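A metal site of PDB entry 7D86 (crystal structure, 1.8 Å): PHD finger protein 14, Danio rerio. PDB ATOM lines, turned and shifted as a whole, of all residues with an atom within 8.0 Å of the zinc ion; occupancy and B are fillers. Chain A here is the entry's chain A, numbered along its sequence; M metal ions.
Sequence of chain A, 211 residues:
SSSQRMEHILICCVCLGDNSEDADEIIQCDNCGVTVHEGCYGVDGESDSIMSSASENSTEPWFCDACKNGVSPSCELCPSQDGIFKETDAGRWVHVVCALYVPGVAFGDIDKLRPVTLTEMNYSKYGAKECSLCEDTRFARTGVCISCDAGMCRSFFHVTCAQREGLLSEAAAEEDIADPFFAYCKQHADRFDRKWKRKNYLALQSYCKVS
Four residues have an atom within 4 Å of the zinc ion: Cys 131, Cys 134, His 158 and Cys 161.
ND1 of His 158 is bound to the zinc ion (2.1 Å). The side-chain sulfur (SG) of Cys 161 is bound to the zinc ion, 2.3 Å away. The zinc ion is bound by SG of Cys 134, 2.4 Å away. SG of Cys 131 is bound to the zinc ion, at 2.4 Å.
A ring nitrogen (NE2) of His 158 sits at hydrogen-bond distance from the backbone carbonyl oxygen (O) of Thr 142 (2.6 Å). SG of Cys 131 lies close to N of Leu 133 (3.3 Å). The backbone NH of Cys 131 sits at hydrogen-bond distance from the backbone carbonyl oxygen of Ala 140, 2.7 Å away. The backbone NH (N) of Cys 131 is in hydrogen-bond range of the side-chain sulfur (SG) of Cys 145, at 3.6 Å.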
ATOM      1  N   LEU A  77     -17.833   7.587   2.192  1.00  0.00           N
ATOM      2  CA  LEU A  77     -16.974   8.339   3.102  1.00  0.00           C
ATOM      3  C   LEU A  77     -15.490   8.152   2.832  1.00  0.00           C
ATOM      4  O   LEU A  77     -14.680   8.790   3.508  1.00  0.00           O
ATOM      5  CB  LEU A  77     -17.264   7.947   4.557  1.00  0.00           C
ATOM      6  CG  LEU A  77     -18.706   8.024   5.053  1.00  0.00           C
ATOM      7  CD1 LEU A  77     -18.778   7.442   6.458  1.00  0.00           C
ATOM      8  CD2 LEU A  77     -19.222   9.471   5.042  1.00  0.00           C
ATOM      9  N   CYS A  78     -15.112   7.299   1.880  1.00  0.00           N
ATOM     10  CA  CYS A  78     -13.705   7.012   1.625  1.00  0.00           C
ATOM     11  C   CYS A  78     -13.582   6.366   0.247  1.00  0.00           C
ATOM     12  O   CYS A  78     -14.588   5.883  -0.307  1.00  0.00           O
ATOM     13  CB  CYS A  78     -13.134   6.079   2.709  1.00  0.00           C
ATOM     14  SG  CYS A  78     -13.497   4.340   2.385  1.00  0.00           S
ATOM     15  N   PRO A  79     -12.384   6.339  -0.331  1.00  0.00           N
ATOM     16  CA  PRO A  79     -12.224   5.785  -1.676  1.00  0.00           C
ATOM     17  C   PRO A  79     -11.977   4.280  -1.738  1.00  0.00           C
ATOM     18  O   PRO A  79     -11.950   3.721  -2.844  1.00  0.00           O
ATOM     19  CB  PRO A  79     -11.000   6.540  -2.220  1.00  0.00           C
ATOM     20  CG  PRO A  79     -10.183   6.825  -1.008  1.00  0.00           C
ATOM     21  CD  PRO A  79     -11.186   7.091   0.107  1.00  0.00           C
ATOM     22  N   SER A  80     -11.809   3.614  -0.602  1.00  0.00           N
ATOM     23  CA  SER A  80     -11.521   2.188  -0.611  1.00  0.00           C
ATOM     24  C   SER A  80     -12.732   1.377  -1.059  1.00  0.00           C
ATOM     25  O   SER A  80     -13.865   1.651  -0.639  1.00  0.00           O
ATOM     26  CB  SER A  80     -11.085   1.718   0.767  1.00  0.00           C
ATOM     27  OG  SER A  80     -11.007   0.303   0.830  1.00  0.00           O
ATOM     28  N   GLU A 130      -8.127  17.096   2.953  1.00  0.00           N
ATOM     29  CA  GLU A 130      -7.312  16.240   2.090  1.00  0.00           C
ATOM     30  C   GLU A 130      -6.688  15.149   2.939  1.00  0.00           C
ATOM     31  O   GLU A 130      -6.075  15.427   3.973  1.00  0.00           O
ATOM     32  CB  GLU A 130      -6.220  17.034   1.373  1.00  0.00           C
ATOM     33  CG  GLU A 130      -5.261  16.147   0.593  1.00  0.00           C
ATOM     34  CD  GLU A 130      -4.331  16.928  -0.318  1.00  0.00           C
ATOM     35  OE1 GLU A 130      -4.224  18.161  -0.152  1.00  0.00           O
ATOM     36  OE2 GLU A 130      -3.720  16.301  -1.212  1.00  0.00           O
ATOM     37  N   CYS A 131      -6.860  13.908   2.496  1.00  0.00           N
ATOM     38  CA  CYS A 131      -6.285  12.776   3.211  1.00  0.00           C
ATOM     39  C   CYS A 131      -4.774  12.739   2.982  1.00  0.00           C
ATOM     40  O   CYS A 131      -4.306  12.722   1.848  1.00  0.00           O
ATOM     41  CB  CYS A 131      -6.919  11.471   2.739  1.00  0.00           C
ATOM     42  SG  CYS A 131      -6.118   9.984   3.387  1.00  0.00           S
ATOM     43  N   SER A 132      -4.018  12.726   4.082  1.00  0.00           N
ATOM     44  CA  SER A 132      -2.561  12.719   3.978  1.00  0.00           C
ATOM     45  C   SER A 132      -1.994  11.333   3.722  1.00  0.00           C
ATOM     46  O   SER A 132      -0.784  11.206   3.497  1.00  0.00           O
ATOM     47  CB  SER A 132      -1.951  13.297   5.250  1.00  0.00           C
ATOM     48  OG  SER A 132      -2.342  12.521   6.378  1.00  0.00           O
ATOM     49  N   LEU A 133      -2.815  10.290   3.772  1.00  0.00           N
ATOM     50  CA  LEU A 133      -2.339   8.918   3.628  1.00  0.00           C
ATOM     51  C   LEU A 133      -2.760   8.239   2.324  1.00  0.00           C
ATOM     52  O   LEU A 133      -2.479   7.048   2.161  1.00  0.00           O
ATOM     53  CB  LEU A 133      -2.830   8.074   4.809  1.00  0.00           C
ATOM     54  CG  LEU A 133      -2.277   8.511   6.167  1.00  0.00           C
ATOM     55  CD1 LEU A 133      -2.910   7.675   7.266  1.00  0.00           C
ATOM     56  CD2 LEU A 133      -0.770   8.360   6.160  1.00  0.00           C
ATOM     57  N   CYS A 134      -3.419   8.955   1.415  1.00  0.00           N
ATOM     58  CA  CYS A 134      -4.001   8.309   0.237  1.00  0.00           C
ATOM     59  C   CYS A 134      -2.916   7.764  -0.686  1.00  0.00           C
ATOM     60  O   CYS A 134      -1.942   8.445  -1.000  1.00  0.00           O
ATOM     61  CB  CYS A 134      -4.884   9.301  -0.513  1.00  0.00           C
ATOM     62  SG  CYS A 134      -6.678   8.952  -0.415  1.00  0.00           S
ATOM     63  N   GLU A 135      -3.084   6.510  -1.119  1.00  0.00           N
ATOM     64  CA  GLU A 135      -2.160   5.936  -2.086  1.00  0.00           C
ATOM     65  C   GLU A 135      -2.358   6.556  -3.465  1.00  0.00           C
ATOM     66  O   GLU A 135      -1.397   6.754  -4.217  1.00  0.00           O
ATOM     67  CB  GLU A 135      -2.342   4.418  -2.165  1.00  0.00           C
ATOM     68  CG  GLU A 135      -2.261   3.719  -0.825  1.00  0.00           C
ATOM     69  CD  GLU A 135      -2.785   2.302  -0.875  1.00  0.00           C
ATOM     70  OE1 GLU A 135      -2.142   1.448  -1.513  1.00  0.00           O
ATOM     71  OE2 GLU A 135      -3.863   2.049  -0.294  1.00  0.00           O
ATOM     72  N   ASP A 136      -3.598   6.874  -3.807  1.00  0.00           N
ATOM     73  CA  ASP A 136      -3.956   7.418  -5.110  1.00  0.00           C
ATOM     74  C   ASP A 136      -4.305   8.887  -4.935  1.00  0.00           C
ATOM     75  O   ASP A 136      -5.312   9.222  -4.294  1.00  0.00           O
ATOM     76  CB  ASP A 136      -5.114   6.643  -5.724  1.00  0.00           C
ATOM     77  CG  ASP A 136      -5.292   6.931  -7.198  1.00  0.00           C
ATOM     78  OD1 ASP A 136      -5.136   8.103  -7.609  1.00  0.00           O
ATOM     79  OD2 ASP A 136      -5.596   5.982  -7.937  1.00  0.00           O
ATOM     80  N   PHE A 139      -7.922  10.689  -5.170  1.00  0.00           N
ATOM     81  CA  PHE A 139      -9.006  10.505  -4.208  1.00  0.00           C
ATOM     82  C   PHE A 139      -8.736  11.148  -2.857  1.00  0.00           C
ATOM     83  O   PHE A 139      -9.557  11.006  -1.943  1.00  0.00           O
ATOM     84  CB  PHE A 139      -9.287   9.012  -4.046  1.00  0.00           C
ATOM     85  CG  PHE A 139      -9.571   8.319  -5.358  1.00  0.00           C
ATOM     86  CD1 PHE A 139     -10.768   8.518  -6.016  1.00  0.00           C
ATOM     87  CD2 PHE A 139      -8.638   7.470  -5.920  1.00  0.00           C
ATOM     88  CE1 PHE A 139     -11.039   7.881  -7.217  1.00  0.00           C
ATOM     89  CE2 PHE A 139      -8.899   6.830  -7.130  1.00  0.00           C
ATOM     90  CZ  PHE A 139     -10.097   7.029  -7.768  1.00  0.00           C
ATOM     91  N   ALA A 140      -7.629  11.881  -2.708  1.00  0.00           N
ATOM     92  CA  ALA A 140      -7.267  12.444  -1.418  1.00  0.00           C
ATOM     93  C   ALA A 140      -8.340  13.396  -0.880  1.00  0.00           C
ATOM     94  O   ALA A 140      -8.456  13.566   0.343  1.00  0.00           O
ATOM     95  CB  ALA A 140      -5.929  13.182  -1.510  1.00  0.00           C
ATOM     96  N   ARG A 141      -9.116  14.020  -1.767  1.00  0.00           N
ATOM     97  CA  ARG A 141     -10.134  14.973  -1.344  1.00  0.00           C
ATOM     98  C   ARG A 141     -11.552  14.427  -1.512  1.00  0.00           C
ATOM     99  O   ARG A 141     -12.495  15.191  -1.713  1.00  0.00           O
ATOM    100  CB  ARG A 141      -9.989  16.300  -2.099  1.00  0.00           C
ATOM    101  CG  ARG A 141      -8.976  17.246  -1.489  1.00  0.00           C
ATOM    102  CD  ARG A 141      -8.895  18.546  -2.270  1.00  0.00           C
ATOM    103  NE  ARG A 141      -7.963  19.482  -1.657  1.00  0.00           N
ATOM    104  CZ  ARG A 141      -6.650  19.474  -1.853  1.00  0.00           C
ATOM    105  NH1 ARG A 141      -5.875  20.368  -1.264  1.00  0.00           N
ATOM    106  NH2 ARG A 141      -6.097  18.553  -2.648  1.00  0.00           N
ATOM    107  N   THR A 142     -11.711  13.124  -1.431  1.00  0.00           N
ATOM    108  CA  THR A 142     -13.032  12.523  -1.489  1.00  0.00           C
ATOM    109  C   THR A 142     -13.472  12.098  -0.098  1.00  0.00           C
ATOM    110  O   THR A 142     -12.657  11.902   0.809  1.00  0.00           O
ATOM    111  CB  THR A 142     -13.056  11.297  -2.412  1.00  0.00           C
ATOM    112  OG1 THR A 142     -12.276  10.255  -1.840  1.00  0.00           O
ATOM    113  CG2 THR A 142     -12.516  11.647  -3.804  1.00  0.00           C
ATOM    114  N   VAL A 144     -14.875  11.684   3.629  1.00  0.00           N
ATOM    115  CA  VAL A 144     -14.745  12.389   4.898  1.00  0.00           C
ATOM    116  C   VAL A 144     -13.487  11.881   5.595  1.00  0.00           C
ATOM    117  O   VAL A 144     -13.286  10.662   5.707  1.00  0.00           O
ATOM    118  CB  VAL A 144     -15.992  12.189   5.785  1.00  0.00           C
ATOM    119  CG1 VAL A 144     -15.790  12.828   7.151  1.00  0.00           C
ATOM    120  CG2 VAL A 144     -17.209  12.799   5.120  1.00  0.00           C
ATOM    121  N   CYS A 145     -12.642  12.804   6.030  1.00  0.00           N
ATOM    122  CA  CYS A 145     -11.449  12.441   6.791  1.00  0.00           C
ATOM    123  C   CYS A 145     -11.722  12.529   8.282  1.00  0.00           C
ATOM    124  O   CYS A 145     -12.574  13.314   8.721  1.00  0.00           O
ATOM    125  CB  CYS A 145     -10.280  13.366   6.441  1.00  0.00           C
ATOM    126  SG  CYS A 145      -9.547  13.097   4.821  1.00  0.00           S
ATOM    127  N   PHE A 156      -4.955  14.637   9.019  1.00  0.00           N
ATOM    128  CA  PHE A 156      -6.218  14.121   8.493  1.00  0.00           C
ATOM    129  C   PHE A 156      -6.004  12.936   7.551  1.00  0.00           C
ATOM    130  O   PHE A 156      -5.045  12.919   6.771  1.00  0.00           O
ATOM    131  CB  PHE A 156      -6.992  15.218   7.761  1.00  0.00           C
ATOM    132  CG  PHE A 156      -7.350  16.380   8.630  1.00  0.00           C
ATOM    133  CD1 PHE A 156      -8.309  16.240   9.622  1.00  0.00           C
ATOM    134  CD2 PHE A 156      -6.720  17.595   8.481  1.00  0.00           C
ATOM    135  CE1 PHE A 156      -8.633  17.323  10.455  1.00  0.00           C
ATOM    136  CE2 PHE A 156      -7.038  18.664   9.305  1.00  0.00           C
ATOM    137  CZ  PHE A 156      -7.996  18.524  10.297  1.00  0.00           C
ATOM    138  N   PHE A 157      -6.931  11.980   7.611  1.00  0.00           N
ATOM    139  CA  PHE A 157      -6.861  10.810   6.757  1.00  0.00           C
ATOM    140  C   PHE A 157      -8.217  10.126   6.706  1.00  0.00           C
ATOM    141  O   PHE A 157      -9.019  10.236   7.639  1.00  0.00           O
ATOM    142  CB  PHE A 157      -5.793   9.811   7.242  1.00  0.00           C
ATOM    143  CG  PHE A 157      -5.537   9.860   8.719  1.00  0.00           C
ATOM    144  CD1 PHE A 157      -6.477   9.410   9.626  1.00  0.00           C
ATOM    145  CD2 PHE A 157      -4.327  10.345   9.211  1.00  0.00           C
ATOM    146  CE1 PHE A 157      -6.244   9.460  11.001  1.00  0.00           C
ATOM    147  CE2 PHE A 157      -4.075  10.387  10.578  1.00  0.00           C
ATOM    148  CZ  PHE A 157      -5.037   9.935  11.473  1.00  0.00           C
ATOM    149  N   HIS A 158      -8.470   9.425   5.608  1.00  0.00           N
ATOM    150  CA  HIS A 158      -9.648   8.568   5.545  1.00  0.00           C
ATOM    151  C   HIS A 158      -9.526   7.468   6.591  1.00  0.00           C
ATOM    152  O   HIS A 158      -8.423   7.035   6.943  1.00  0.00           O
ATOM    153  CB  HIS A 158      -9.789   7.914   4.164  1.00  0.00           C
ATOM    154  CG  HIS A 158     -10.015   8.886   3.060  1.00  0.00           C
ATOM    155  ND1 HIS A 158      -9.103   9.091   2.043  1.00  0.00           N
ATOM    156  CD2 HIS A 158     -11.056   9.715   2.799  1.00  0.00           C
ATOM    157  CE1 HIS A 158      -9.578   9.999   1.208  1.00  0.00           C
ATOM    158  NE2 HIS A 158     -10.760  10.391   1.653  1.00  0.00           N
ATOM    159  N   VAL A 159     -10.684   6.980   7.068  1.00  0.00           N
ATOM    160  CA  VAL A 159     -10.679   5.930   8.074  1.00  0.00           C
ATOM    161  C   VAL A 159      -9.984   4.682   7.546  1.00  0.00           C
ATOM    162  O   VAL A 159      -9.196   4.047   8.254  1.00  0.00           O
ATOM    163  CB  VAL A 159     -12.111   5.613   8.535  1.00  0.00           C
ATOM    164  CG1 VAL A 159     -12.100   4.443   9.512  1.00  0.00           C
ATOM    165  CG2 VAL A 159     -12.745   6.844   9.159  1.00  0.00           C
ATOM    166  N   THR A 160     -10.257   4.309   6.292  1.00  0.00           N
ATOM    167  CA  THR A 160      -9.680   3.090   5.743  1.00  0.00           C
ATOM    168  C   THR A 160      -8.208   3.267   5.387  1.00  0.00           C
ATOM    169  O   THR A 160      -7.444   2.301   5.414  1.00  0.00           O
ATOM    170  CB  THR A 160     -10.463   2.628   4.515  1.00  0.00           C
ATOM    171  OG1 THR A 160     -10.684   3.733   3.631  1.00  0.00           O
ATOM    172  CG2 THR A 160     -11.814   2.060   4.946  1.00  0.00           C
ATOM    173  N   CYS A 161      -7.794   4.492   5.028  1.00  0.00           N
ATOM    174  CA  CYS A 161      -6.385   4.758   4.827  1.00  0.00           C
ATOM    175  C   CYS A 161      -5.615   4.647   6.140  1.00  0.00           C
ATOM    176  O   CYS A 161      -4.530   4.055   6.191  1.00  0.00           O
ATOM    177  CB  CYS A 161      -6.196   6.139   4.196  1.00  0.00           C
ATOM    178  SG  CYS A 161      -6.778   6.268   2.457  1.00  0.00           S
ATOM    179  N   ALA A 162      -6.195   5.180   7.218  1.00  0.00           N
ATOM    180  CA  ALA A 162      -5.597   5.001   8.537  1.00  0.00           C
ATOM    181  C   ALA A 162      -5.608   3.528   8.944  1.00  0.00           C
ATOM    182  O   ALA A 162      -4.654   3.031   9.554  1.00  0.00           O
ATOM    183  CB  ALA A 162      -6.329   5.860   9.578  1.00  0.00           C
ATOM    184  N   ARG A 164      -5.299   0.957   7.062  1.00  0.00           N
ATOM    185  CA  ARG A 164      -4.235   0.275   6.329  1.00  0.00           C
ATOM    186  C   ARG A 164      -2.890   0.502   6.985  1.00  0.00           C
ATOM    187  O   ARG A 164      -2.025  -0.387   6.990  1.00  0.00           O
ATOM    188  CB  ARG A 164      -4.221   0.763   4.879  1.00  0.00           C
ATOM    189  CG  ARG A 164      -3.131   0.192   4.017  1.00  0.00           C
ATOM    190  CD  ARG A 164      -3.052   0.932   2.680  1.00  0.00           C
ATOM    191  NE  ARG A 164      -2.377   2.217   2.835  1.00  0.00           N
ATOM    192  CZ  ARG A 164      -2.952   3.402   2.601  1.00  0.00           C
ATOM    193  NH1 ARG A 164      -4.205   3.467   2.180  1.00  0.00           N
ATOM    194  NH2 ARG A 164      -2.254   4.514   2.780  1.00  0.00           N
HETATM  195 ZN    ZN M   1      -7.119   8.482   1.851  1.00  0.00          ZN
